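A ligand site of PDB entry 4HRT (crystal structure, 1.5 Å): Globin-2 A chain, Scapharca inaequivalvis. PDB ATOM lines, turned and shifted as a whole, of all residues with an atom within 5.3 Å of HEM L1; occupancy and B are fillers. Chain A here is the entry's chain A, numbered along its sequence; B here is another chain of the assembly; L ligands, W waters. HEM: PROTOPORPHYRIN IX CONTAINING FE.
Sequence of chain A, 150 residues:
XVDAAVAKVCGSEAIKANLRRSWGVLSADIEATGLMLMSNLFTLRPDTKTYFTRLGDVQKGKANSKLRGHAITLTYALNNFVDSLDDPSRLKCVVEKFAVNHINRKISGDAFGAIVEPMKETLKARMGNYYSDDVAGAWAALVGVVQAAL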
ATOM      1  N   LEU A  37      15.351  -6.217  17.910  1.00  0.00           N
ATOM      2  CA  LEU A  37      15.476  -6.131  19.368  1.00  0.00           C
ATOM      3  C   LEU A  37      14.151  -6.463  20.060  1.00  0.00           C
ATOM      4  O   LEU A  37      14.128  -7.256  21.003  1.00  0.00           O
ATOM      5  CB  LEU A  37      15.995  -4.753  19.797  1.00  0.00           C
ATOM      6  CG  LEU A  37      16.172  -4.532  21.312  1.00  0.00           C
ATOM      7  CD1 LEU A  37      17.148  -5.517  21.949  1.00  0.00           C
ATOM      8  CD2 LEU A  37      16.603  -3.105  21.585  1.00  0.00           C
ATOM      9  N   LEU A  41      13.274  -9.519  22.573  1.00  0.00           N
ATOM     10  CA  LEU A  41      12.706  -9.248  23.901  1.00  0.00           C
ATOM     11  C   LEU A  41      11.496 -10.137  24.170  1.00  0.00           C
ATOM     12  O   LEU A  41      11.426 -10.779  25.220  1.00  0.00           O
ATOM     13  CB  LEU A  41      12.326  -7.767  24.065  1.00  0.00           C
ATOM     14  CG  LEU A  41      11.672  -7.350  25.399  1.00  0.00           C
ATOM     15  CD1 LEU A  41      12.610  -7.583  26.570  1.00  0.00           C
ATOM     16  CD2 LEU A  41      11.235  -5.899  25.353  1.00  0.00           C
ATOM     17  N   THR A  48       7.668  -9.848  29.790  1.00  0.00           N
ATOM     18  CA  THR A  48       7.622  -8.395  29.587  1.00  0.00           C
ATOM     19  C   THR A  48       6.454  -7.924  28.716  1.00  0.00           C
ATOM     20  O   THR A  48       6.176  -6.726  28.656  1.00  0.00           O
ATOM     21  CB  THR A  48       8.948  -7.843  28.976  1.00  0.00           C
ATOM     22  OG1 THR A  48       9.120  -8.354  27.653  1.00  0.00           O
ATOM     23  CG2 THR A  48      10.147  -8.208  29.843  1.00  0.00           C
ATOM     24  N   TYR A  51       3.728  -5.294  29.862  1.00  0.00           N
ATOM     25  CA  TYR A  51       3.920  -3.836  29.830  1.00  0.00           C
ATOM     26  C   TYR A  51       3.449  -3.188  28.522  1.00  0.00           C
ATOM     27  O   TYR A  51       3.333  -1.969  28.442  1.00  0.00           O
ATOM     28  CB  TYR A  51       5.409  -3.472  30.041  1.00  0.00           C
ATOM     29  CG  TYR A  51       5.945  -3.845  31.417  1.00  0.00           C
ATOM     30  CD1 TYR A  51       5.694  -3.030  32.528  1.00  0.00           C
ATOM     31  CD2 TYR A  51       6.680  -5.011  31.608  1.00  0.00           C
ATOM     32  CE1 TYR A  51       6.180  -3.363  33.785  1.00  0.00           C
ATOM     33  CE2 TYR A  51       7.168  -5.353  32.869  1.00  0.00           C
ATOM     34  CZ  TYR A  51       6.908  -4.537  33.959  1.00  0.00           C
ATOM     35  OH  TYR A  51       7.392  -4.861  35.212  1.00  0.00           O
ATOM     36  N   PHE A  52       3.166  -4.011  27.504  1.00  0.00           N
ATOM     37  CA  PHE A  52       2.944  -3.526  26.131  1.00  0.00           C
ATOM     38  C   PHE A  52       1.540  -3.781  25.583  1.00  0.00           C
ATOM     39  O   PHE A  52       1.352  -3.919  24.368  1.00  0.00           O
ATOM     40  CB  PHE A  52       3.999  -4.125  25.176  1.00  0.00           C
ATOM     41  CG  PHE A  52       5.424  -3.680  25.463  1.00  0.00           C
ATOM     42  CD1 PHE A  52       5.925  -2.507  24.906  1.00  0.00           C
ATOM     43  CD2 PHE A  52       6.247  -4.429  26.294  1.00  0.00           C
ATOM     44  CE1 PHE A  52       7.242  -2.104  25.156  1.00  0.00           C
ATOM     45  CE2 PHE A  52       7.560  -4.044  26.555  1.00  0.00           C
ATOM     46  CZ  PHE A  52       8.049  -2.876  25.993  1.00  0.00           C
ATOM     47  N   ARG A  54      -0.884  -1.843  24.973  1.00  0.00           N
ATOM     48  CA  ARG A  54      -1.341  -0.894  23.945  1.00  0.00           C
ATOM     49  C   ARG A  54      -0.951  -1.329  22.536  1.00  0.00           C
ATOM     50  O   ARG A  54      -1.647  -1.012  21.566  1.00  0.00           O
ATOM     51  CB  ARG A  54      -0.826   0.529  24.238  1.00  0.00           C
ATOM     52  CG  ARG A  54      -1.502   1.621  23.401  1.00  0.00           C
ATOM     53  CD  ARG A  54      -0.764   2.968  23.445  1.00  0.00           C
ATOM     54  NE  ARG A  54       0.524   2.953  22.735  1.00  0.00           N
ATOM     55  CZ  ARG A  54       0.687   3.151  21.425  1.00  0.00           C
ATOM     56  NH1 ARG A  54      -0.358   3.391  20.647  1.00  0.00           N
ATOM     57  NH2 ARG A  54       1.909   3.128  20.904  1.00  0.00           N
ATOM     58  N   LEU A  55       0.170  -2.047  22.416  1.00  0.00           N
ATOM     59  CA  LEU A  55       0.691  -2.444  21.105  1.00  0.00           C
ATOM     60  C   LEU A  55      -0.082  -3.570  20.412  1.00  0.00           C
ATOM     61  O   LEU A  55       0.100  -3.774  19.218  1.00  0.00           O
ATOM     62  CB  LEU A  55       2.196  -2.766  21.187  1.00  0.00           C
ATOM     63  CG  LEU A  55       3.150  -1.703  21.745  1.00  0.00           C
ATOM     64  CD1 LEU A  55       4.587  -2.170  21.560  1.00  0.00           C
ATOM     65  CD2 LEU A  55       2.943  -0.343  21.073  1.00  0.00           C
ATOM     66  N   HIS A  70       6.909   2.038  17.725  1.00  0.00           N
ATOM     67  CA  HIS A  70       7.674   1.915  18.949  1.00  0.00           C
ATOM     68  C   HIS A  70       9.124   1.454  18.687  1.00  0.00           C
ATOM     69  O   HIS A  70      10.068   2.051  19.216  1.00  0.00           O
ATOM     70  CB  HIS A  70       7.004   0.978  19.962  1.00  0.00           C
ATOM     71  CG  HIS A  70       7.869   0.702  21.155  1.00  0.00           C
ATOM     72  ND1 HIS A  70       8.079   1.643  22.153  1.00  0.00           N
ATOM     73  CD2 HIS A  70       8.632  -0.362  21.473  1.00  0.00           C
ATOM     74  CE1 HIS A  70       8.904   1.142  23.051  1.00  0.00           C
ATOM     75  NE2 HIS A  70       9.258  -0.070  22.662  1.00  0.00           N
ATOM     76  N   THR A  73      11.163   4.251  17.165  1.00  0.00           N
ATOM     77  CA  THR A  73      11.367   5.318  18.151  1.00  0.00           C
ATOM     78  C   THR A  73      12.372   4.947  19.238  1.00  0.00           C
ATOM     79  O   THR A  73      13.192   5.786  19.648  1.00  0.00           O
ATOM     80  CB  THR A  73       9.992   5.774  18.692  1.00  0.00           C
ATOM     81  OG1 THR A  73       9.238   6.254  17.584  1.00  0.00           O
ATOM     82  CG2 THR A  73      10.106   6.885  19.734  1.00  0.00           C
ATOM     83  N   LEU A  74      12.351   3.694  19.682  1.00  0.00           N
ATOM     84  CA  LEU A  74      13.303   3.199  20.684  1.00  0.00           C
ATOM     85  C   LEU A  74      14.750   3.481  20.264  1.00  0.00           C
ATOM     86  O   LEU A  74      15.582   3.857  21.088  1.00  0.00           O
ATOM     87  CB  LEU A  74      13.065   1.700  20.948  1.00  0.00           C
ATOM     88  CG  LEU A  74      14.053   0.903  21.803  1.00  0.00           C
ATOM     89  CD1 LEU A  74      13.360  -0.273  22.474  1.00  0.00           C
ATOM     90  CD2 LEU A  74      15.249   0.441  20.967  1.00  0.00           C
ATOM     91  N   ALA A  77      16.418   6.896  21.137  1.00  0.00           N
ATOM     92  CA  ALA A  77      16.954   7.013  22.498  1.00  0.00           C
ATOM     93  C   ALA A  77      18.380   6.432  22.533  1.00  0.00           C
ATOM     94  O   ALA A  77      19.285   7.059  23.108  1.00  0.00           O
ATOM     95  CB  ALA A  77      16.061   6.311  23.521  1.00  0.00           C
ATOM     96  N   LEU A  78      18.589   5.261  21.920  1.00  0.00           N
ATOM     97  CA  LEU A  78      19.932   4.674  21.823  1.00  0.00           C
ATOM     98  C   LEU A  78      20.888   5.634  21.109  1.00  0.00           C
ATOM     99  O   LEU A  78      22.020   5.787  21.542  1.00  0.00           O
ATOM    100  CB  LEU A  78      19.901   3.299  21.123  1.00  0.00           C
ATOM    101  CG  LEU A  78      19.099   2.202  21.839  1.00  0.00           C
ATOM    102  CD1 LEU A  78      19.198   0.901  21.048  1.00  0.00           C
ATOM    103  CD2 LEU A  78      19.568   2.003  23.282  1.00  0.00           C
ATOM    104  N   PHE A  81      21.811   8.336  23.526  1.00  0.00           N
ATOM    105  CA  PHE A  81      22.778   7.801  24.530  1.00  0.00           C
ATOM    106  C   PHE A  81      24.195   7.724  23.945  1.00  0.00           C
ATOM    107  O   PHE A  81      25.157   8.162  24.591  1.00  0.00           O
ATOM    108  CB  PHE A  81      22.385   6.388  25.027  1.00  0.00           C
ATOM    109  CG  PHE A  81      21.085   6.300  25.790  1.00  0.00           C
ATOM    110  CD1 PHE A  81      20.397   7.419  26.267  1.00  0.00           C
ATOM    111  CD2 PHE A  81      20.576   5.042  26.055  1.00  0.00           C
ATOM    112  CE1 PHE A  81      19.187   7.274  26.969  1.00  0.00           C
ATOM    113  CE2 PHE A  81      19.379   4.880  26.761  1.00  0.00           C
ATOM    114  CZ  PHE A  81      18.695   6.005  27.221  1.00  0.00           C
ATOM    115  N   PHE A  98      14.962  10.254  30.174  1.00  0.00           N
ATOM    116  CA  PHE A  98      14.454   8.988  29.631  1.00  0.00           C
ATOM    117  C   PHE A  98      13.737   8.157  30.690  1.00  0.00           C
ATOM    118  O   PHE A  98      12.714   7.521  30.392  1.00  0.00           O
ATOM    119  CB  PHE A  98      15.651   8.221  29.056  1.00  0.00           C
ATOM    120  CG  PHE A  98      15.356   6.804  28.639  1.00  0.00           C
ATOM    121  CD1 PHE A  98      15.496   5.751  29.547  1.00  0.00           C
ATOM    122  CD2 PHE A  98      14.968   6.518  27.343  1.00  0.00           C
ATOM    123  CE1 PHE A  98      15.234   4.440  29.184  1.00  0.00           C
ATOM    124  CE2 PHE A  98      14.717   5.210  26.952  1.00  0.00           C
ATOM    125  CZ  PHE A  98      14.857   4.170  27.865  1.00  0.00           C
ATOM    126  N   ASN A 101       9.324   8.528  32.145  1.00  0.00           N
ATOM    127  CA  ASN A 101       8.136   7.758  31.723  1.00  0.00           C
ATOM    128  C   ASN A 101       8.228   6.284  32.095  1.00  0.00           C
ATOM    129  O   ASN A 101       7.208   5.640  32.333  1.00  0.00           O
ATOM    130  CB  ASN A 101       7.887   7.865  30.215  1.00  0.00           C
ATOM    131  CG  ASN A 101       7.512   9.257  29.759  1.00  0.00           C
ATOM    132  OD1 ASN A 101       7.056  10.103  30.542  1.00  0.00           O
ATOM    133  ND2 ASN A 101       7.678   9.508  28.469  1.00  0.00           N
ATOM    134  N   HIS A 102       9.441   5.745  32.147  1.00  0.00           N
ATOM    135  CA  HIS A 102       9.642   4.340  32.542  1.00  0.00           C
ATOM    136  C   HIS A 102       9.312   4.114  34.026  1.00  0.00           C
ATOM    137  O   HIS A 102       8.707   3.100  34.381  1.00  0.00           O
ATOM    138  CB  HIS A 102      11.044   3.838  32.118  1.00  0.00           C
ATOM    139  CG  HIS A 102      11.210   3.661  30.638  1.00  0.00           C
ATOM    140  ND1 HIS A 102      11.598   4.688  29.807  1.00  0.00           N
ATOM    141  CD2 HIS A 102      11.016   2.582  29.840  1.00  0.00           C
ATOM    142  CE1 HIS A 102      11.630   4.248  28.557  1.00  0.00           C
ATOM    143  NE2 HIS A 102      11.288   2.971  28.553  1.00  0.00           N
ATOM    144  N   ARG A 105       5.560   4.089  34.309  1.00  0.00           N
ATOM    145  CA  ARG A 105       5.009   2.799  33.872  1.00  0.00           C
ATOM    146  C   ARG A 105       5.337   1.668  34.857  1.00  0.00           C
ATOM    147  O   ARG A 105       5.034   0.497  34.593  1.00  0.00           O
ATOM    148  CB  ARG A 105       5.472   2.479  32.430  1.00  0.00           C
ATOM    149  CG  ARG A 105       4.911   3.439  31.385  1.00  0.00           C
ATOM    150  CD  ARG A 105       5.190   3.043  29.949  1.00  0.00           C
ATOM    151  NE  ARG A 105       6.547   3.394  29.620  1.00  0.00           N
ATOM    152  CZ  ARG A 105       6.923   4.441  28.876  1.00  0.00           C
ATOM    153  NH1 ARG A 105       6.026   5.269  28.322  1.00  0.00           N
ATOM    154  NH2 ARG A 105       8.216   4.652  28.681  1.00  0.00           N
ATOM    155  N   ILE A 107       8.263   0.365  35.781  1.00  0.00           N
ATOM    156  CA  ILE A 107       9.329  -0.527  35.310  1.00  0.00           C
ATOM    157  C   ILE A 107      10.544  -0.332  36.218  1.00  0.00           C
ATOM    158  O   ILE A 107      11.204   0.710  36.179  1.00  0.00           O
ATOM    159  CB  ILE A 107       9.691  -0.254  33.839  1.00  0.00           C
ATOM    160  CG1 ILE A 107       8.463  -0.456  32.951  1.00  0.00           C
ATOM    161  CG2 ILE A 107      10.844  -1.146  33.397  1.00  0.00           C
ATOM    162  CD1 ILE A 107       8.568   0.247  31.617  1.00  0.00           C
ATOM    163  N   ALA A 111      13.332  -5.092  36.150  1.00  0.00           N
ATOM    164  CA  ALA A 111      12.497  -5.301  34.969  1.00  0.00           C
ATOM    165  C   ALA A 111      13.146  -4.796  33.683  1.00  0.00           C
ATOM    166  O   ALA A 111      13.139  -5.487  32.659  1.00  0.00           O
ATOM    167  CB  ALA A 111      11.119  -4.677  35.152  1.00  0.00           C
ATOM    168  N   PHE A 112      13.710  -3.597  33.741  1.00  0.00           N
ATOM    169  CA  PHE A 112      14.366  -2.997  32.581  1.00  0.00           C
ATOM    170  C   PHE A 112      15.523  -3.869  32.128  1.00  0.00           C
ATOM    171  O   PHE A 112      15.786  -3.972  30.917  1.00  0.00           O
ATOM    172  CB  PHE A 112      14.841  -1.582  32.880  1.00  0.00           C
ATOM    173  CG  PHE A 112      15.196  -0.783  31.658  1.00  0.00           C
ATOM    174  CD1 PHE A 112      14.220  -0.029  30.993  1.00  0.00           C
ATOM    175  CD2 PHE A 112      16.494  -0.784  31.146  1.00  0.00           C
ATOM    176  CE1 PHE A 112      14.543   0.711  29.868  1.00  0.00           C
ATOM    177  CE2 PHE A 112      16.814  -0.047  30.013  1.00  0.00           C
ATOM    178  CZ  PHE A 112      15.834   0.701  29.363  1.00  0.00           C
ATOM    179  N   ALA A 114      15.653  -6.866  31.719  1.00  0.00           N
ATOM    180  CA  ALA A 114      15.209  -7.917  30.784  1.00  0.00           C
ATOM    181  C   ALA A 114      15.703  -7.679  29.365  1.00  0.00           C
ATOM    182  O   ALA A 114      15.749  -8.615  28.556  1.00  0.00           O
ATOM    183  CB  ALA A 114      13.687  -8.047  30.797  1.00  0.00           C
ATOM    184  N   ILE A 115      16.051  -6.429  29.044  1.00  0.00           N
ATOM    185  CA  ILE A 115      16.545  -6.094  27.706  1.00  0.00           C
ATOM    186  C   ILE A 115      17.959  -6.629  27.387  1.00  0.00           C
ATOM    187  O   ILE A 115      18.331  -6.687  26.221  1.00  0.00           O
ATOM    188  CB  ILE A 115      16.488  -4.559  27.410  1.00  0.00           C
ATOM    189  CG1 ILE A 115      16.478  -4.287  25.892  1.00  0.00           C
ATOM    190  CG2 ILE A 115      17.625  -3.826  28.109  1.00  0.00           C
ATOM    191  CD1 ILE A 115      15.176  -4.642  25.195  1.00  0.00           C
ATOM    192  N   MET A 119      19.362  -7.853  23.783  1.00  0.00           N
ATOM    193  CA  MET A 119      20.331  -6.985  23.107  1.00  0.00           C
ATOM    194  C   MET A 119      21.558  -7.796  22.682  1.00  0.00           C
ATOM    195  O   MET A 119      22.032  -7.625  21.557  1.00  0.00           O
ATOM    196  CB  MET A 119      20.769  -5.795  23.978  1.00  0.00           C
ATOM    197  CG  MET A 119      21.812  -4.895  23.308  1.00  0.00           C
ATOM    198  SD  MET A 119      21.274  -4.194  21.730  1.00  0.00           S
ATOM    199  CE  MET A 119      20.402  -2.748  22.311  1.00  0.00           C
ATOM    200  N   VAL A 143      23.057  -0.017  29.852  1.00  0.00           N
ATOM    201  CA  VAL A 143      21.746  -0.342  30.443  1.00  0.00           C
ATOM    202  C   VAL A 143      21.790  -0.149  31.971  1.00  0.00           C
ATOM    203  O   VAL A 143      20.810   0.312  32.583  1.00  0.00           O
ATOM    204  CB  VAL A 143      21.284  -1.762  30.039  1.00  0.00           C
ATOM    205  CG1 VAL A 143      20.106  -2.216  30.889  1.00  0.00           C
ATOM    206  CG2 VAL A 143      20.924  -1.801  28.568  1.00  0.00           C
ATOM    207  N   LYS B  99       2.900   7.254  17.226  1.00  0.00           N
ATOM    208  CA  LYS B  99       3.641   6.852  18.429  1.00  0.00           C
ATOM    209  C   LYS B  99       3.985   8.081  19.290  1.00  0.00           C
ATOM    210  O   LYS B  99       3.726   8.104  20.492  1.00  0.00           O
ATOM    211  CB  LYS B  99       4.908   6.073  18.033  1.00  0.00           C
ATOM    212  CG  LYS B  99       5.984   5.937  19.111  1.00  0.00           C
ATOM    213  CD  LYS B  99       5.558   5.026  20.260  1.00  0.00           C
ATOM    214  CE  LYS B  99       6.672   4.957  21.316  1.00  0.00           C
ATOM    215  NZ  LYS B  99       6.366   4.105  22.512  1.00  0.00           N
ATOM    216  N   ASN B 103       1.939  10.094  24.186  1.00  0.00           N
ATOM    217  CA  ASN B 103       2.205  10.820  25.442  1.00  0.00           C
ATOM    218  C   ASN B 103       1.677  12.252  25.436  1.00  0.00           C
ATOM    219  O   ASN B 103       1.288  12.788  26.483  1.00  0.00           O
ATOM    220  CB  ASN B 103       3.711  10.877  25.759  1.00  0.00           C
ATOM    221  CG  ASN B 103       4.323   9.514  26.085  1.00  0.00           C
ATOM    222  OD1 ASN B 103       5.532   9.325  25.937  1.00  0.00           O
ATOM    223  ND2 ASN B 103       3.504   8.565  26.517  1.00  0.00           N
HETATM  224  CHA HEM L   1       8.386   3.619  25.499  1.00  0.00           C
HETATM  225  CHB HEM L   1      13.192   3.518  24.790  1.00  0.00           C
HETATM  226  CHC HEM L   1      13.439  -0.680  27.280  1.00  0.00           C
HETATM  227  CHD HEM L   1       8.717  -0.364  28.287  1.00  0.00           C
HETATM  228  C1A HEM L   1       9.686   3.999  25.141  1.00  0.00           C
HETATM  229  C2A HEM L   1      10.010   5.143  24.368  1.00  0.00           C
HETATM  230  C3A HEM L   1      11.372   5.109  24.152  1.00  0.00           C
HETATM  231  C4A HEM L   1      11.859   3.949  24.818  1.00  0.00           C
HETATM  232  CMA HEM L   1      12.219   6.136  23.395  1.00  0.00           C
HETATM  233  CAA HEM L   1       9.075   6.248  23.869  1.00  0.00           C
HETATM  234  CBA HEM L   1       9.065   7.454  24.838  1.00  0.00           C
HETATM  235  CGA HEM L   1       8.398   7.095  26.141  1.00  0.00           C
HETATM  236  O1A HEM L   1       7.157   6.969  26.184  1.00  0.00           O
HETATM  237  O2A HEM L   1       9.054   6.941  27.186  1.00  0.00           O
HETATM  238  C1B HEM L   1      13.660   2.306  25.337  1.00  0.00           C
HETATM  239  C2B HEM L   1      15.019   1.826  25.196  1.00  0.00           C
HETATM  240  C3B HEM L   1      15.086   0.635  25.881  1.00  0.00           C
HETATM  241  C4B HEM L   1      13.730   0.419  26.470  1.00  0.00           C
HETATM  242  CMB HEM L   1      16.124   2.496  24.406  1.00  0.00           C
HETATM  243  CAB HEM L   1      16.220  -0.310  26.074  1.00  0.00           C
HETATM  244  CBB HEM L   1      17.190  -0.478  25.174  1.00  0.00           C
HETATM  245  C1C HEM L   1      12.178  -0.957  27.819  1.00  0.00           C
HETATM  246  C2C HEM L   1      11.849  -2.145  28.511  1.00  0.00           C
HETATM  247  C3C HEM L   1      10.474  -2.056  28.820  1.00  0.00           C
HETATM  248  C4C HEM L   1      10.027  -0.802  28.281  1.00  0.00           C
HETATM  249  CMC HEM L   1      12.810  -3.260  28.855  1.00  0.00           C
HETATM  250  CAC HEM L   1       9.612  -3.019  29.552  1.00  0.00           C
HETATM  251  CBC HEM L   1      10.066  -3.897  30.454  1.00  0.00           C
HETATM  252  C1D HEM L   1       8.273   0.701  27.488  1.00  0.00           C
HETATM  253  C2D HEM L   1       6.810   0.948  27.301  1.00  0.00           C
HETATM  254  C3D HEM L   1       6.719   2.058  26.535  1.00  0.00           C
HETATM  255  C4D HEM L   1       8.130   2.459  26.245  1.00  0.00           C
HETATM  256  CMD HEM L   1       5.686   0.142  27.896  1.00  0.00           C
HETATM  257  CAD HEM L   1       5.455   2.710  26.017  1.00  0.00           C
HETATM  258  CBD HEM L   1       5.027   1.840  24.804  1.00  0.00           C
HETATM  259  CGD HEM L   1       3.832   2.297  23.973  1.00  0.00           C
HETATM  260  O1D HEM L   1       2.677   2.121  24.393  1.00  0.00           O
HETATM  261  O2D HEM L   1       3.959   2.822  22.844  1.00  0.00           O
HETATM  262  NA  HEM L   1      10.831   3.302  25.478  1.00  0.00           N
HETATM  263  NB  HEM L   1      12.985   1.521  26.209  1.00  0.00           N
HETATM  264  NC  HEM L   1      11.086  -0.136  27.706  1.00  0.00           N
HETATM  265  ND  HEM L   1       9.052   1.691  26.935  1.00  0.00           N
HETATM  266 FE   HEM L   1      10.961   1.635  26.625  1.00  0.00          FE
HETATM  267  CHA HEM L   2       7.942  15.477  26.234  1.00  0.00           C
HETATM  268  CHB HEM L   2       9.140  16.071  21.576  1.00  0.00           C
HETATM  269  CHC HEM L   2       6.174  19.969  21.386  1.00  0.00           C
HETATM  270  CHD HEM L   2       4.852  19.213  25.990  1.00  0.00           C
HETATM  271  C1A HEM L   2       8.488  15.249  24.974  1.00  0.00           C
HETATM  272  C2A HEM L   2       9.413  14.208  24.658  1.00  0.00           C
HETATM  273  C3A HEM L   2       9.766  14.380  23.331  1.00  0.00           C
HETATM  274  C4A HEM L   2       9.054  15.529  22.862  1.00  0.00           C
HETATM  275  CMA HEM L   2      10.719  13.514  22.492  1.00  0.00           C
HETATM  276  CAA HEM L   2       9.891  13.093  25.561  1.00  0.00           C
HETATM  277  CBA HEM L   2       9.059  11.822  25.293  1.00  0.00           C
HETATM  278  CGA HEM L   2       7.666  12.019  25.859  1.00  0.00           C
HETATM  279  O1A HEM L   2       7.508  12.072  27.105  1.00  0.00           O
HETATM  280  O2A HEM L   2       6.679  12.158  25.097  1.00  0.00           O
HETATM  281  C1B HEM L   2       8.481  17.245  21.136  1.00  0.00           C
HETATM  282  C2B HEM L   2       8.677  17.857  19.849  1.00  0.00           C
HETATM  283  C3B HEM L   2       7.848  18.949  19.784  1.00  0.00           C
HETATM  284  C4B HEM L   2       7.142  19.001  21.089  1.00  0.00           C
HETATM  285  CMB HEM L   2       9.600  17.365  18.772  1.00  0.00           C
HETATM  286  CAB HEM L   2       7.654  19.939  18.693  1.00  0.00           C
HETATM  287  CBB HEM L   2       8.544  20.195  17.745  1.00  0.00           C
HETATM  288  C1C HEM L   2       5.544  20.116  22.633  1.00  0.00           C
HETATM  289  C2C HEM L   2       4.769  21.235  23.023  1.00  0.00           C
HETATM  290  C3C HEM L   2       4.389  21.011  24.349  1.00  0.00           C
HETATM  291  C4C HEM L   2       4.948  19.745  24.729  1.00  0.00           C
HETATM  292  CMC HEM L   2       4.413  22.410  22.142  1.00  0.00           C
HETATM  293  CAC HEM L   2       3.547  21.839  25.273  1.00  0.00           C
HETATM  294  CBC HEM L   2       3.267  23.132  25.121  1.00  0.00           C
HETATM  295  C1D HEM L   2       5.697  18.179  26.416  1.00  0.00           C
HETATM  296  C2D HEM L   2       5.771  17.813  27.853  1.00  0.00           C
HETATM  297  C3D HEM L   2       6.634  16.781  27.936  1.00  0.00           C
HETATM  298  C4D HEM L   2       7.078  16.543  26.518  1.00  0.00           C
HETATM  299  CMD HEM L   2       5.020  18.475  28.999  1.00  0.00           C
HETATM  300  CAD HEM L   2       7.091  16.075  29.219  1.00  0.00           C
HETATM  301  CBD HEM L   2       8.226  16.979  29.791  1.00  0.00           C
HETATM  302  CGD HEM L   2       8.965  16.464  31.015  1.00  0.00           C
HETATM  303  O1D HEM L   2      10.167  16.081  30.939  1.00  0.00           O
HETATM  304  O2D HEM L   2       8.403  16.438  32.146  1.00  0.00           O
HETATM  305  NA  HEM L   2       8.194  15.988  23.840  1.00  0.00           N
HETATM  306  NB  HEM L   2       7.465  17.865  21.754  1.00  0.00           N
HETATM  307  NC  HEM L   2       5.600  19.188  23.660  1.00  0.00           N
HETATM  308  ND  HEM L   2       6.392  17.303  25.601  1.00  0.00           N
HETATM  309 FE   HEM L   2       6.865  17.537  23.739  1.00  0.00          FE
HETATM  310  O   HOH W   1      10.939  -1.361  24.712  1.00  0.00           O
HETATM  311  O   HOH W   2      11.553   7.995  27.674  1.00  0.00           O
HETATM  312  O   HOH W   3       2.307  -0.423  25.561  1.00  0.00           O
HETATM  313  O   HOH W   4       5.505   6.260  24.188  1.00  0.00           O
HETATM  314  O   HOH W   5       3.399   0.049  30.448  1.00  0.00           O
HETATM  315  O   HOH W   6       1.593   4.096  26.312  1.00  0.00           O
HETATM  316  O   HOH W   7       1.561   1.687  27.022  1.00  0.00           O
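Water W4 bridges O1A of HEM L1 (2.7 Å) and NZ of Lys 99 of chain B (2.9 Å).
Water W2 bridges O2A of HEM L1 (2.8 Å) and O of Phe 98 (3.0 Å).
Water W3 bridges an oxygen (O1D) of HEM L1 (2.8 Å) and the backbone carbonyl oxygen (O) of Tyr 51 (3.4 Å).
Merely in contact with HEM L1: Tyr 51 (3.2 Å), Phe 52 (3.5 Å), Leu 55 (3.8 Å), His 70 (3.5 Å), Thr 73 (3.9 Å), Leu 74 (3.6 Å), Ala 77 (3.8 Å), Leu 78 (3.7 Å), Phe 98 (3.1 Å), Ile 107 (3.4 Å), Phe 112 (3.1 Å) and Ile 115 (3.9 Å).
OD1 of Asn 103 of chain B lies within hydrogen-bond range of ND2 of Asn 101.
The backbone carbonyl oxygen (O) of His 102 is in hydrogen-bond range of the backbone NH (N) of Ile 107.
The backbone carbonyl oxygen (O) of Phe 98 is in hydrogen-bond range of a ring nitrogen (ND1) of His 102 (3.1 Å).
A ring nitrogen (ND1) of His 70 sits at hydrogen-bond distance from the side-chain amino group of Lys 99 of chain B (3.0 Å).
O1A of HEM L1 sits close to OD1 of Asn 103 of chain B (2.9 Å).
The side-chain amide nitrogen of Asn 101 is in hydrogen-bond range of an oxygen (O2A) of HEM L1 (3.2 Å).
NH2 of Arg 54 is in salt-bridge range of O2D of HEM L1 (2.8 Å).
A ring nitrogen (NE2) of His 102 is bound to an iron atom (FE) of HEM L1 (2.4 Å).
The guanidinium group (NH2) of Arg 105 is in salt-bridge range of an oxygen (O2A) of HEM L1, at 2.9 Å.
The side-chain amino group (NZ) of Lys 99 of chain B lies within salt-bridge range of an oxygen (O2D) of HEM L1, at 2.7 Å.
The side-chain amide oxygen (OD1) of Asn 103 of chain B sits close to an oxygen (O2A) of HEM L2, at 3.2 Å.
ND2 of Asn 101 is in hydrogen-bond range of O1A of HEM L2.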
